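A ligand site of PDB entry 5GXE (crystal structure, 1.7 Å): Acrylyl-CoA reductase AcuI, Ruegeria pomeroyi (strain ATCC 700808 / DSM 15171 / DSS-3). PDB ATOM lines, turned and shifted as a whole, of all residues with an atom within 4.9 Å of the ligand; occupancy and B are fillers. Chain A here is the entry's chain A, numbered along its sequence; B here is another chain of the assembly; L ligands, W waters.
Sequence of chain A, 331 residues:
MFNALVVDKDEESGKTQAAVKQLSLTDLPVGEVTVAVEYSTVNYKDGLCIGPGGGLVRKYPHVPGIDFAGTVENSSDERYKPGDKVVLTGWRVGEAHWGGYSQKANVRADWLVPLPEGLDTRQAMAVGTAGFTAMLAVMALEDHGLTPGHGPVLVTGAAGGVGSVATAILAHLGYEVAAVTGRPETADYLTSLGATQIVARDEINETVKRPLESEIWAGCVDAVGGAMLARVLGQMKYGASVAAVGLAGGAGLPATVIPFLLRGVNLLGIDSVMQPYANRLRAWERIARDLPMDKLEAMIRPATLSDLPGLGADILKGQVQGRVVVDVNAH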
ATOM      1  N   VAL A  42      19.405   1.501   2.252  1.00  0.00           N
ATOM      2  CA  VAL A  42      19.705   0.569   3.337  1.00  0.00           C
ATOM      3  C   VAL A  42      21.149   0.131   3.168  1.00  0.00           C
ATOM      4  O   VAL A  42      21.466  -0.612   2.227  1.00  0.00           O
ATOM      5  CB  VAL A  42      18.781  -0.639   3.365  1.00  0.00           C
ATOM      6  CG1 VAL A  42      19.147  -1.557   4.527  1.00  0.00           C
ATOM      7  CG2 VAL A  42      17.320  -0.226   3.461  1.00  0.00           C
ATOM      8  N   ASN A  43      22.013   0.575   4.064  1.00  0.00           N
ATOM      9  CA  ASN A  43      23.389   0.107   4.172  1.00  0.00           C
ATOM     10  C   ASN A  43      23.474  -0.981   5.227  1.00  0.00           C
ATOM     11  O   ASN A  43      22.607  -1.102   6.090  1.00  0.00           O
ATOM     12  CB  ASN A  43      24.323   1.248   4.556  1.00  0.00           C
ATOM     13  CG  ASN A  43      24.388   2.321   3.503  1.00  0.00           C
ATOM     14  OD1 ASN A  43      25.134   2.199   2.526  1.00  0.00           O
ATOM     15  ND2 ASN A  43      23.603   3.382   3.688  1.00  0.00           N
ATOM     16  N   TYR A  44      24.567  -1.755   5.197  1.00  0.00           N
ATOM     17  CA  TYR A  44      24.780  -2.735   6.255  1.00  0.00           C
ATOM     18  C   TYR A  44      24.662  -2.085   7.623  1.00  0.00           C
ATOM     19  O   TYR A  44      23.968  -2.600   8.515  1.00  0.00           O
ATOM     20  CB  TYR A  44      26.156  -3.386   6.082  1.00  0.00           C
ATOM     21  CG  TYR A  44      26.437  -4.520   7.042  1.00  0.00           C
ATOM     22  CD1 TYR A  44      26.992  -4.274   8.298  1.00  0.00           C
ATOM     23  CD2 TYR A  44      26.188  -5.833   6.691  1.00  0.00           C
ATOM     24  CE1 TYR A  44      27.266  -5.306   9.170  1.00  0.00           C
ATOM     25  CE2 TYR A  44      26.477  -6.876   7.555  1.00  0.00           C
ATOM     26  CZ  TYR A  44      27.018  -6.600   8.794  1.00  0.00           C
ATOM     27  OH  TYR A  44      27.292  -7.632   9.667  1.00  0.00           O
ATOM     28  N   LYS A  45      25.305  -0.930   7.801  1.00  0.00           N
ATOM     29  CA  LYS A  45      25.246  -0.243   9.085  1.00  0.00           C
ATOM     30  C   LYS A  45      23.825   0.138   9.462  1.00  0.00           C
ATOM     31  O   LYS A  45      23.470   0.118  10.647  1.00  0.00           O
ATOM     32  CB  LYS A  45      26.138   0.998   9.056  1.00  0.00           C
ATOM     33  CG  LYS A  45      26.097   1.818  10.356  1.00  0.00           C
ATOM     34  CD  LYS A  45      27.439   2.484  10.642  1.00  0.00           C
ATOM     35  CE  LYS A  45      27.848   3.408   9.528  1.00  0.00           C
ATOM     36  NZ  LYS A  45      29.106   4.139   9.872  1.00  0.00           N
ATOM     37  N   THR A 129      25.947   5.462   0.883  1.00  0.00           N
ATOM     38  CA  THR A 129      27.242   5.252   1.535  1.00  0.00           C
ATOM     39  C   THR A 129      27.993   4.076   0.923  1.00  0.00           C
ATOM     40  O   THR A 129      29.223   4.141   0.737  1.00  0.00           O
ATOM     41  CB  THR A 129      27.039   5.052   3.047  1.00  0.00           C
ATOM     42  OG1 THR A 129      27.002   6.344   3.678  1.00  0.00           O
ATOM     43  CG2 THR A 129      28.178   4.219   3.677  1.00  0.00           C
ATOM     44  N   ALA A 130      27.283   2.995   0.581  1.00  0.00           N
ATOM     45  CA  ALA A 130      27.929   1.824  -0.010  1.00  0.00           C
ATOM     46  C   ALA A 130      28.696   2.183  -1.275  1.00  0.00           C
ATOM     47  O   ALA A 130      29.887   1.851  -1.429  1.00  0.00           O
ATOM     48  CB  ALA A 130      26.898   0.745  -0.311  1.00  0.00           C
ATOM     49  N   THR A 133      31.525   4.683  -0.860  1.00  0.00           N
ATOM     50  CA  THR A 133      32.717   4.073  -0.288  1.00  0.00           C
ATOM     51  C   THR A 133      33.429   3.197  -1.315  1.00  0.00           C
ATOM     52  O   THR A 133      34.665   3.146  -1.348  1.00  0.00           O
ATOM     53  CB  THR A 133      32.332   3.260   0.950  1.00  0.00           C
ATOM     54  OG1 THR A 133      31.573   4.105   1.833  1.00  0.00           O
ATOM     55  CG2 THR A 133      33.563   2.771   1.683  1.00  0.00           C
ATOM     56  N   GLY A 157      32.242 -10.017  -1.643  1.00  0.00           N
ATOM     57  CA  GLY A 157      30.843  -9.754  -1.299  1.00  0.00           C
ATOM     58  C   GLY A 157      30.133  -9.028  -2.416  1.00  0.00           C
ATOM     59  O   GLY A 157      29.390  -8.066  -2.176  1.00  0.00           O
ATOM     60  N   ALA A 158      30.343  -9.505  -3.637  1.00  0.00           N
ATOM     61  CA  ALA A 158      30.085  -8.700  -4.827  1.00  0.00           C
ATOM     62  C   ALA A 158      28.593  -8.467  -5.071  1.00  0.00           C
ATOM     63  O   ALA A 158      28.230  -7.481  -5.711  1.00  0.00           O
ATOM     64  CB  ALA A 158      30.712  -9.359  -6.057  1.00  0.00           C
ATOM     65  N   ALA A 159      27.738  -9.366  -4.601  1.00  0.00           N
ATOM     66  CA  ALA A 159      26.312  -9.231  -4.869  1.00  0.00           C
ATOM     67  C   ALA A 159      25.640  -8.203  -3.982  1.00  0.00           C
ATOM     68  O   ALA A 159      24.492  -7.823  -4.264  1.00  0.00           O
ATOM     69  CB  ALA A 159      25.613 -10.583  -4.714  1.00  0.00           C
ATOM     70  N   GLY A 160      26.320  -7.746  -2.929  1.00  0.00           N
ATOM     71  CA  GLY A 160      25.814  -6.726  -2.044  1.00  0.00           C
ATOM     72  C   GLY A 160      26.024  -5.326  -2.588  1.00  0.00           C
ATOM     73  O   GLY A 160      26.278  -5.117  -3.778  1.00  0.00           O
ATOM     74  N   GLY A 161      25.939  -4.344  -1.687  1.00  0.00           N
ATOM     75  CA  GLY A 161      25.930  -2.940  -2.081  1.00  0.00           C
ATOM     76  C   GLY A 161      27.280  -2.417  -2.517  1.00  0.00           C
ATOM     77  O   GLY A 161      27.430  -1.952  -3.657  1.00  0.00           O
ATOM     78  N   VAL A 162      28.253  -2.418  -1.598  1.00  0.00           N
ATOM     79  CA  VAL A 162      29.620  -2.022  -1.942  1.00  0.00           C
ATOM     80  C   VAL A 162      30.106  -2.820  -3.136  1.00  0.00           C
ATOM     81  O   VAL A 162      30.677  -2.279  -4.089  1.00  0.00           O
ATOM     82  CB  VAL A 162      30.551  -2.214  -0.746  1.00  0.00           C
ATOM     83  CG1 VAL A 162      32.006  -1.974  -1.149  1.00  0.00           C
ATOM     84  CG2 VAL A 162      30.150  -1.271   0.400  1.00  0.00           C
ATOM     85  N   GLY A 163      29.883  -4.133  -3.082  1.00  0.00           N
ATOM     86  CA  GLY A 163      30.400  -5.014  -4.118  1.00  0.00           C
ATOM     87  C   GLY A 163      29.796  -4.737  -5.477  1.00  0.00           C
ATOM     88  O   GLY A 163      30.503  -4.740  -6.479  1.00  0.00           O
ATOM     89  N   VAL A 180      33.648 -12.062  -6.010  1.00  0.00           N
ATOM     90  CA  VAL A 180      33.474 -13.136  -5.031  1.00  0.00           C
ATOM     91  C   VAL A 180      32.059 -13.061  -4.464  1.00  0.00           C
ATOM     92  O   VAL A 180      31.662 -12.035  -3.893  1.00  0.00           O
ATOM     93  CB  VAL A 180      34.507 -13.008  -3.899  1.00  0.00           C
ATOM     94  CG1 VAL A 180      34.312 -14.125  -2.881  1.00  0.00           C
ATOM     95  CG2 VAL A 180      35.931 -13.073  -4.466  1.00  0.00           C
ATOM     96  N   THR A 181      31.298 -14.152  -4.598  1.00  0.00           N
ATOM     97  CA  THR A 181      29.951 -14.171  -4.029  1.00  0.00           C
ATOM     98  C   THR A 181      29.669 -15.519  -3.390  1.00  0.00           C
ATOM     99  O   THR A 181      30.153 -16.557  -3.860  1.00  0.00           O
ATOM    100  CB  THR A 181      28.881 -13.865  -5.088  1.00  0.00           C
ATOM    101  OG1 THR A 181      27.593 -13.758  -4.449  1.00  0.00           O
ATOM    102  CG2 THR A 181      28.806 -14.951  -6.152  1.00  0.00           C
ATOM    103  N   GLY A 182      28.905 -15.491  -2.307  1.00  0.00           N
ATOM    104  CA  GLY A 182      28.349 -16.679  -1.688  1.00  0.00           C
ATOM    105  C   GLY A 182      26.963 -17.027  -2.180  1.00  0.00           C
ATOM    106  O   GLY A 182      26.342 -17.978  -1.679  1.00  0.00           O
ATOM    107  N   ARG A 183      26.452 -16.277  -3.158  1.00  0.00           N
ATOM    108  CA  ARG A 183      25.129 -16.511  -3.749  1.00  0.00           C
ATOM    109  C   ARG A 183      25.366 -16.824  -5.220  1.00  0.00           C
ATOM    110  O   ARG A 183      25.318 -15.926  -6.070  1.00  0.00           O
ATOM    111  CB  ARG A 183      24.222 -15.299  -3.559  1.00  0.00           C
ATOM    112  CG  ARG A 183      23.787 -15.074  -2.124  1.00  0.00           C
ATOM    113  CD  ARG A 183      22.883 -13.848  -2.017  1.00  0.00           C
ATOM    114  NE  ARG A 183      23.664 -12.624  -1.867  1.00  0.00           N
ATOM    115  CZ  ARG A 183      23.119 -11.421  -1.782  1.00  0.00           C
ATOM    116  NH1 ARG A 183      21.797 -11.279  -1.846  1.00  0.00           N
ATOM    117  NH2 ARG A 183      23.886 -10.346  -1.616  1.00  0.00           N
ATOM    118  N   ARG A 201      32.511 -17.987  -2.889  1.00  0.00           N
ATOM    119  CA  ARG A 201      32.975 -17.585  -1.559  1.00  0.00           C
ATOM    120  C   ARG A 201      33.773 -18.692  -0.873  1.00  0.00           C
ATOM    121  O   ARG A 201      34.839 -18.435  -0.294  1.00  0.00           O
ATOM    122  CB  ARG A 201      31.786 -17.198  -0.677  1.00  0.00           C
ATOM    123  CG  ARG A 201      32.170 -16.907   0.767  1.00  0.00           C
ATOM    124  CD  ARG A 201      30.946 -16.840   1.668  1.00  0.00           C
ATOM    125  NE  ARG A 201      30.028 -15.795   1.250  1.00  0.00           N
ATOM    126  CZ  ARG A 201      28.832 -15.615   1.798  1.00  0.00           C
ATOM    127  NH1 ARG A 201      28.457 -16.418   2.778  1.00  0.00           N
ATOM    128  NH2 ARG A 201      28.038 -14.627   1.383  1.00  0.00           N
ATOM    129  N   ALA A 223      34.746  -5.892   0.969  1.00  0.00           N
ATOM    130  CA  ALA A 223      33.588  -5.620   1.810  1.00  0.00           C
ATOM    131  C   ALA A 223      33.371  -6.674   2.903  1.00  0.00           C
ATOM    132  O   ALA A 223      32.464  -6.524   3.723  1.00  0.00           O
ATOM    133  CB  ALA A 223      32.321  -5.533   0.951  1.00  0.00           C
ATOM    134  N   VAL A 224      34.211  -7.709   2.928  1.00  0.00           N
ATOM    135  CA  VAL A 224      33.983  -8.895   3.754  1.00  0.00           C
ATOM    136  C   VAL A 224      34.904  -8.941   4.971  1.00  0.00           C
ATOM    137  O   VAL A 224      34.457  -9.281   6.070  1.00  0.00           O
ATOM    138  CB  VAL A 224      34.166 -10.164   2.880  1.00  0.00           C
ATOM    139  CG1 VAL A 224      34.170 -11.427   3.737  1.00  0.00           C
ATOM    140  CG2 VAL A 224      33.082 -10.215   1.798  1.00  0.00           C
ATOM    141  N   MET A 228      38.473 -14.263   4.977  1.00  0.00           N
ATOM    142  CA  MET A 228      38.621 -14.030   3.541  1.00  0.00           C
ATOM    143  C   MET A 228      39.694 -12.984   3.262  1.00  0.00           C
ATOM    144  O   MET A 228      40.572 -13.190   2.409  1.00  0.00           O
ATOM    145  CB  MET A 228      37.289 -13.601   2.913  1.00  0.00           C
ATOM    146  CG  MET A 228      37.385 -13.490   1.413  1.00  0.00           C
ATOM    147  SD  MET A 228      35.892 -12.865   0.615  1.00  0.00           S
ATOM    148  CE  MET A 228      34.734 -14.203   0.931  1.00  0.00           C
ATOM    149  N   VAL A 245      37.163  -2.132   3.297  1.00  0.00           N
ATOM    150  CA  VAL A 245      35.907  -1.414   3.415  1.00  0.00           C
ATOM    151  C   VAL A 245      35.011  -2.029   4.494  1.00  0.00           C
ATOM    152  O   VAL A 245      34.412  -1.299   5.279  1.00  0.00           O
ATOM    153  CB  VAL A 245      35.174  -1.369   2.058  1.00  0.00           C
ATOM    154  CG1 VAL A 245      33.714  -0.848   2.214  1.00  0.00           C
ATOM    155  CG2 VAL A 245      35.941  -0.527   1.067  1.00  0.00           C
ATOM    156  N   GLY A 246      34.922  -3.353   4.564  1.00  0.00           N
ATOM    157  CA  GLY A 246      33.880  -3.981   5.350  1.00  0.00           C
ATOM    158  C   GLY A 246      34.337  -5.146   6.212  1.00  0.00           C
ATOM    159  O   GLY A 246      35.503  -5.568   6.169  1.00  0.00           O
ATOM    160  N   LEU A 247      33.377  -5.665   6.985  1.00  0.00           N
ATOM    161  CA  LEU A 247      33.580  -6.757   7.922  1.00  0.00           C
ATOM    162  C   LEU A 247      32.395  -7.724   7.905  1.00  0.00           C
ATOM    163  O   LEU A 247      32.133  -8.409   8.896  1.00  0.00           O
ATOM    164  CB  LEU A 247      33.787  -6.219   9.343  1.00  0.00           C
ATOM    165  CG  LEU A 247      32.914  -5.043   9.806  1.00  0.00           C
ATOM    166  CD1 LEU A 247      31.381  -5.294   9.769  1.00  0.00           C
ATOM    167  CD2 LEU A 247      33.341  -4.664  11.195  1.00  0.00           C
ATOM    168  N   ALA A 248      31.688  -7.792   6.782  1.00  0.00           N
ATOM    169  CA  ALA A 248      30.509  -8.651   6.690  1.00  0.00           C
ATOM    170  C   ALA A 248      30.851 -10.114   6.987  1.00  0.00           C
ATOM    171  O   ALA A 248      29.982 -10.863   7.465  1.00  0.00           O
ATOM    172  CB  ALA A 248      29.870  -8.515   5.318  1.00  0.00           C
ATOM    173  N   GLY A 249      32.085 -10.527   6.722  1.00  0.00           N
ATOM    174  CA  GLY A 249      32.572 -11.859   7.026  1.00  0.00           C
ATOM    175  C   GLY A 249      33.293 -11.982   8.360  1.00  0.00           C
ATOM    176  O   GLY A 249      33.840 -13.050   8.664  1.00  0.00           O
ATOM    177  N   ILE A 270      39.585   2.273   4.555  1.00  0.00           N
ATOM    178  CA  ILE A 270      38.659   3.228   3.945  1.00  0.00           C
ATOM    179  C   ILE A 270      37.617   3.605   4.987  1.00  0.00           C
ATOM    180  O   ILE A 270      36.896   2.736   5.493  1.00  0.00           O
ATOM    181  CB  ILE A 270      37.988   2.643   2.704  1.00  0.00           C
ATOM    182  CG1 ILE A 270      39.033   2.098   1.729  1.00  0.00           C
ATOM    183  CG2 ILE A 270      37.102   3.707   2.032  1.00  0.00           C
ATOM    184  CD1 ILE A 270      40.037   3.127   1.249  1.00  0.00           C
ATOM    185  N   ASP A 271      37.530   4.905   5.301  1.00  0.00           N
ATOM    186  CA  ASP A 271      36.486   5.423   6.189  1.00  0.00           C
ATOM    187  C   ASP A 271      35.649   6.435   5.429  1.00  0.00           C
ATOM    188  O   ASP A 271      36.136   7.512   5.084  1.00  0.00           O
ATOM    189  CB  ASP A 271      37.060   6.069   7.442  1.00  0.00           C
ATOM    190  CG  ASP A 271      35.988   6.803   8.233  1.00  0.00           C
ATOM    191  OD1 ASP A 271      34.914   6.208   8.415  1.00  0.00           O
ATOM    192  OD2 ASP A 271      36.205   7.969   8.614  1.00  0.00           O
ATOM    193  N   SER A 272      34.383   6.106   5.178  1.00  0.00           N
ATOM    194  CA  SER A 272      33.502   7.051   4.518  1.00  0.00           C
ATOM    195  C   SER A 272      32.947   8.091   5.481  1.00  0.00           C
ATOM    196  O   SER A 272      32.542   9.176   5.028  1.00  0.00           O
ATOM    197  CB  SER A 272      32.325   6.317   3.890  1.00  0.00           C
ATOM    198  OG  SER A 272      31.525   5.710   4.894  1.00  0.00           O
ATOM    199  N   VAL A 273      32.916   7.795   6.773  1.00  0.00           N
ATOM    200  CA  VAL A 273      31.995   8.512   7.665  1.00  0.00           C
ATOM    201  C   VAL A 273      32.421   9.961   7.834  1.00  0.00           C
ATOM    202  O   VAL A 273      31.571  10.867   7.853  1.00  0.00           O
ATOM    203  CB  VAL A 273      31.881   7.805   9.023  1.00  0.00           C
ATOM    204  CG1 VAL A 273      30.903   8.545   9.926  1.00  0.00           C
ATOM    205  CG2 VAL A 273      31.447   6.364   8.828  1.00  0.00           C
ATOM    206  N   ILE A 315      19.662  -7.528   5.453  1.00  0.00           N
ATOM    207  CA  ILE A 315      20.995  -7.159   5.008  1.00  0.00           C
ATOM    208  C   ILE A 315      22.038  -7.710   5.984  1.00  0.00           C
ATOM    209  O   ILE A 315      23.131  -8.110   5.566  1.00  0.00           O
ATOM    210  CB  ILE A 315      21.113  -5.640   4.800  1.00  0.00           C
ATOM    211  CG1 ILE A 315      22.323  -5.335   3.897  1.00  0.00           C
ATOM    212  CG2 ILE A 315      21.234  -4.896   6.123  1.00  0.00           C
ATOM    213  CD1 ILE A 315      22.373  -3.886   3.413  1.00  0.00           C
ATOM    214  N   GLY A 318      23.104 -11.024   4.887  1.00  0.00           N
ATOM    215  CA  GLY A 318      23.637 -11.119   3.542  1.00  0.00           C
ATOM    216  C   GLY A 318      22.608 -11.415   2.477  1.00  0.00           C
ATOM    217  O   GLY A 318      22.966 -11.948   1.423  1.00  0.00           O
ATOM    218  N   VAL A 320      20.434  -9.154   0.941  1.00  0.00           N
ATOM    219  CA  VAL A 320      20.053  -8.044   0.067  1.00  0.00           C
ATOM    220  C   VAL A 320      21.026  -8.004  -1.107  1.00  0.00           C
ATOM    221  O   VAL A 320      22.245  -7.917  -0.908  1.00  0.00           O
ATOM    222  CB  VAL A 320      20.012  -6.700   0.819  1.00  0.00           C
ATOM    223  CG1 VAL A 320      19.681  -5.564  -0.140  1.00  0.00           C
ATOM    224  CG2 VAL A 320      18.966  -6.765   1.915  1.00  0.00           C
ATOM    225  N   GLY A 322      22.332  -5.964  -4.395  1.00  0.00           N
ATOM    226  CA  GLY A 322      22.349  -4.629  -4.993  1.00  0.00           C
ATOM    227  C   GLY A 322      22.133  -3.538  -3.958  1.00  0.00           C
ATOM    228  O   GLY A 322      22.719  -3.579  -2.872  1.00  0.00           O
ATOM    229  N   LEU B 261      38.946   0.260   9.136  1.00  0.00           N
ATOM    230  CA  LEU B 261      37.637   0.723   8.701  1.00  0.00           C
ATOM    231  C   LEU B 261      37.211   1.982   9.438  1.00  0.00           C
ATOM    232  O   LEU B 261      36.554   2.860   8.855  1.00  0.00           O
ATOM    233  CB  LEU B 261      36.578  -0.354   8.925  1.00  0.00           C
ATOM    234  CG  LEU B 261      36.860  -1.744   8.353  1.00  0.00           C
ATOM    235  CD1 LEU B 261      35.571  -2.562   8.396  1.00  0.00           C
ATOM    236  CD2 LEU B 261      37.454  -1.684   6.949  1.00  0.00           C
HETATM  237  P1  LIG L   1      25.852  -5.837   1.956  1.00  0.00           P
HETATM  238  O1  LIG L   1      25.007  -5.349   0.864  1.00  0.00           O
HETATM  239  O2  LIG L   1      25.201  -6.879   2.873  1.00  0.00           O
HETATM  240  O3  LIG L   1      27.124  -6.420   1.270  1.00  0.00           O
HETATM  241  C1  LIG L   1      27.916  -7.424   1.938  1.00  0.00           C
HETATM  242  C2  LIG L   1      28.106  -8.708   1.166  1.00  0.00           C
HETATM  243  O4  LIG L   1      29.115  -9.443   1.778  1.00  0.00           O
HETATM  244  C3  LIG L   1      26.937  -9.601   1.254  1.00  0.00           C
HETATM  245  O5  LIG L   1      25.842  -9.230   0.429  1.00  0.00           O
HETATM  246  C4  LIG L   1      27.520 -10.839   0.895  1.00  0.00           C
HETATM  247  O6  LIG L   1      27.752 -10.882  -0.507  1.00  0.00           O
HETATM  248  C5  LIG L   1      28.811 -10.788   1.605  1.00  0.00           C
HETATM  249  N1  LIG L   1      28.735 -11.465   2.899  1.00  0.00           N
HETATM  250  C6  LIG L   1      27.840 -11.312   3.879  1.00  0.00           C
HETATM  251  N2  LIG L   1      28.166 -12.134   4.900  1.00  0.00           N
HETATM  252  C7  LIG L   1      29.287 -12.799   4.547  1.00  0.00           C
HETATM  253  C8  LIG L   1      30.093 -13.764   5.169  1.00  0.00           C
HETATM  254  N3  LIG L   1      29.751 -14.248   6.489  1.00  0.00           N
HETATM  255  N4  LIG L   1      31.176 -14.240   4.541  1.00  0.00           N
HETATM  256  C9  LIG L   1      31.492 -13.801   3.323  1.00  0.00           C
HETATM  257  N5  LIG L   1      30.751 -12.881   2.681  1.00  0.00           N
HETATM  258  C10 LIG L   1      29.651 -12.362   3.274  1.00  0.00           C
HETATM  259  O7  LIG L   1      26.349  -4.666   2.858  1.00  0.00           O
HETATM  260  P2  LIG L   1      26.992  -3.258   2.295  1.00  0.00           P
HETATM  261  O8  LIG L   1      26.042  -2.128   2.650  1.00  0.00           O
HETATM  262  O9  LIG L   1      27.369  -3.385   0.849  1.00  0.00           O
HETATM  263  O10 LIG L   1      28.251  -3.054   3.216  1.00  0.00           O
HETATM  264  C11 LIG L   1      29.286  -4.045   3.131  1.00  0.00           C
HETATM  265  C12 LIG L   1      30.281  -4.025   4.207  1.00  0.00           C
HETATM  266  O11 LIG L   1      31.029  -2.798   4.055  1.00  0.00           O
HETATM  267  C13 LIG L   1      29.625  -3.969   5.523  1.00  0.00           C
HETATM  268  O12 LIG L   1      30.390  -4.644   6.437  1.00  0.00           O
HETATM  269  C14 LIG L   1      29.573  -2.545   5.845  1.00  0.00           C
HETATM  270  O13 LIG L   1      29.551  -2.335   7.204  1.00  0.00           O
HETATM  271  C15 LIG L   1      30.866  -2.097   5.253  1.00  0.00           C
HETATM  272  N6  LIG L   1      31.004  -0.641   5.016  1.00  0.00           N
HETATM  273  C16 LIG L   1      31.896   0.299   5.596  1.00  0.00           C
HETATM  274  C17 LIG L   1      31.977   1.685   5.073  1.00  0.00           C
HETATM  275  C18 LIG L   1      33.163   2.484   5.517  1.00  0.00           C
HETATM  276  O14 LIG L   1      33.115   3.656   5.604  1.00  0.00           O
HETATM  277  N7  LIG L   1      34.349   1.735   5.864  1.00  0.00           N
HETATM  278  C19 LIG L   1      31.018   2.213   4.063  1.00  0.00           C
HETATM  279  C20 LIG L   1      30.020   1.198   3.601  1.00  0.00           C
HETATM  280  C21 LIG L   1      30.081  -0.229   4.018  1.00  0.00           C
HETATM  281  P3  LIG L   1      27.613 -12.223  -1.371  1.00  0.00           P
HETATM  282  O15 LIG L   1      27.910 -11.827  -2.808  1.00  0.00           O
HETATM  283  O16 LIG L   1      28.612 -13.223  -0.862  1.00  0.00           O
HETATM  284  O17 LIG L   1      26.198 -12.728  -1.243  1.00  0.00           O
HETATM  285  O   HOH W   1      23.423  -8.396   1.641  1.00  0.00           O
HETATM  286  O   HOH W   2      24.237  -1.690   0.437  1.00  0.00           O
HETATM  287  O   HOH W   3      31.146 -13.478  -0.149  1.00  0.00           O
HETATM  288  O   HOH W   4      25.104 -13.616   1.064  1.00  0.00           O
HETATM  289  O   HOH W   5      29.094  -5.563  -0.760  1.00  0.00           O
HETATM  290  O   HOH W   6      27.115   0.422   2.977  1.00  0.00           O
HETATM  291  O   HOH W   7      22.822  -4.077  -0.154  1.00  0.00           O
HETATM  292  O   HOH W   8      27.369   0.112   5.882  1.00  0.00           O
HETATM  293  O   HOH W   9      25.808  -8.757   4.616  1.00  0.00           O
HETATM  294  O   HOH W  10      25.811 -12.316   7.065  1.00  0.00           O
HETATM  295  O   HOH W  11      31.712 -16.132   7.613  1.00  0.00           O
HETATM  296  O   HOH W  12      29.631   0.496   7.962  1.00  0.00           O
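The side-chain hydroxyl (OG1) of Thr 181 sits at hydrogen-bond distance from the backbone NH (N) of Arg 183, at 3.1 Å. O of Thr 181 sits at hydrogen-bond distance from N of Arg 201 (2.9 Å). The guanidinium group of Arg 183 is in hydrogen-bond range of the backbone carbonyl oxygen of Val 320. The side-chain hydroxyl (OG1) of Thr 133 lies close to the side-chain hydroxyl (OG) of Ser 272, at 3.5 Å. The backbone carbonyl oxygen (O) of Thr 129 sits at hydrogen-bond distance from the side-chain hydroxyl (OG1) of Thr 133 (2.6 Å). The backbone carbonyl oxygen of Ala 159 lies within hydrogen-bond range of the backbone NH of Gly 322 (2.9 Å). The backbone NH (N) of Leu 247 sits at hydrogen-bond distance from the backbone carbonyl oxygen (O) of Ala 223 (3.5 Å). The backbone carbonyl oxygen (O) of Val 180 sits at hydrogen-bond distance from the backbone NH (N) of Ala 158 (2.9 Å).
An oxygen (O15) of the ligand sits at hydrogen-bond distance from the side-chain hydroxyl (OG1) of Thr 181 (2.6 Å). The guanidinium group (NE) of Arg 183 is in salt-bridge range of an oxygen (O17) of the ligand (2.6 Å). O14 of the ligand lies within hydrogen-bond range of N of Ser 272. An oxygen (O14) of the ligand lies within hydrogen-bond range of the side-chain hydroxyl (OG) of Ser 272, 2.7 Å away. An oxygen (O16) of the ligand is in hydrogen-bond range of the backbone NH (N) of Gly 182. NH2 of Arg 201 lies within salt-bridge range of O16 of the ligand (2.7 Å). The backbone carbonyl oxygen (O) of Ile 270 lies within hydrogen-bond range of a nitrogen (N7) of the ligand. An oxygen (O9) of the ligand sits at hydrogen-bond distance from the backbone NH of Val 162 (2.8 Å). An oxygen (O1) of the ligand lies within hydrogen-bond range of the backbone NH of Gly 161 (2.9 Å). The backbone NH of Tyr 44 lies within hydrogen-bond range of an oxygen (O8) of the ligand (3.0 Å). O of Val 245 lies close to N7 of the ligand, at 3.1 Å. The backbone NH (N) of Ala 159 sits at hydrogen-bond distance from an oxygen (O15) of the ligand, at 3.0 Å. The backbone NH of Leu 247 sits at hydrogen-bond distance from an oxygen (O12) of the ligand (3.2 Å). O12 of the ligand is in hydrogen-bond range of N of Ala 248, 3.4 Å away. The backbone NH (N) of Ala 158 is in hydrogen-bond range of an oxygen (O15) of the ligand, at 3.5 Å.
CA of Asn 43 touches O8 of the ligand, 3.8 Å away. CG2 of Thr 129 touches C19 of the ligand, at 3.5 Å. Thr 133 touches the ligand (OG1 to C19, 3.0 Å). Gly 157 touches the ligand (CA to O6, 3.4 Å). CA of Gly 160 touches O1 of the ligand, 3.3 Å away. Val 180 touches the ligand (O to O15, 3.9 Å). Ala 223 touches the ligand. Val 224 touches the ligand (CG1 to C9, 3.6 Å). Gly 246 touches the ligand. Gly 249 touches the ligand. Asp 271 touches the ligand. Ile 315 touches the ligand (CG1 to O2, 3.4 Å). O of Leu 261 of chain B touches N7 of the ligand, at 3.9 Å. Hydrophobic or aromatic side chains within 4 Å of the ligand: Tyr 44, Ala 159, Val 162, Val 224, Val 245, Leu 247, Ala 248 and Ile 315. Of the 36 residues printed, 27 come within 4 Å of the ligand.
Water W9 bridges O2 of the ligand (2.6 Å) and O of Ile 315 (2.9 Å). Water W4 lies within hydrogen-bond range of O17 of the ligand (2.7 Å), O of Gly 318 (2.7 Å), NH2 of Arg 201 (3.1 Å) and NE of Arg 183 (3.4 Å). Water W7 lies within hydrogen-bond range of an oxygen (O1) of the ligand (2.7 Å), the backbone carbonyl oxygen of Gly 322 (2.8 Å) and the backbone NH of Gly 161 (3.5 Å). Water W6 lies within hydrogen-bond range of OD1 of Asn 43 and O8 of the ligand. Water W2 bridges an oxygen (O8) of the ligand (2.9 Å) and the backbone carbonyl oxygen of Val 42 (3.5 Å). Water W5 lies within hydrogen-bond range of N of Gly 163 (2.8 Å), O of Gly 157 (2.9 Å), O3 of the ligand (3.0 Å) and N of Val 162 (3.4 Å).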
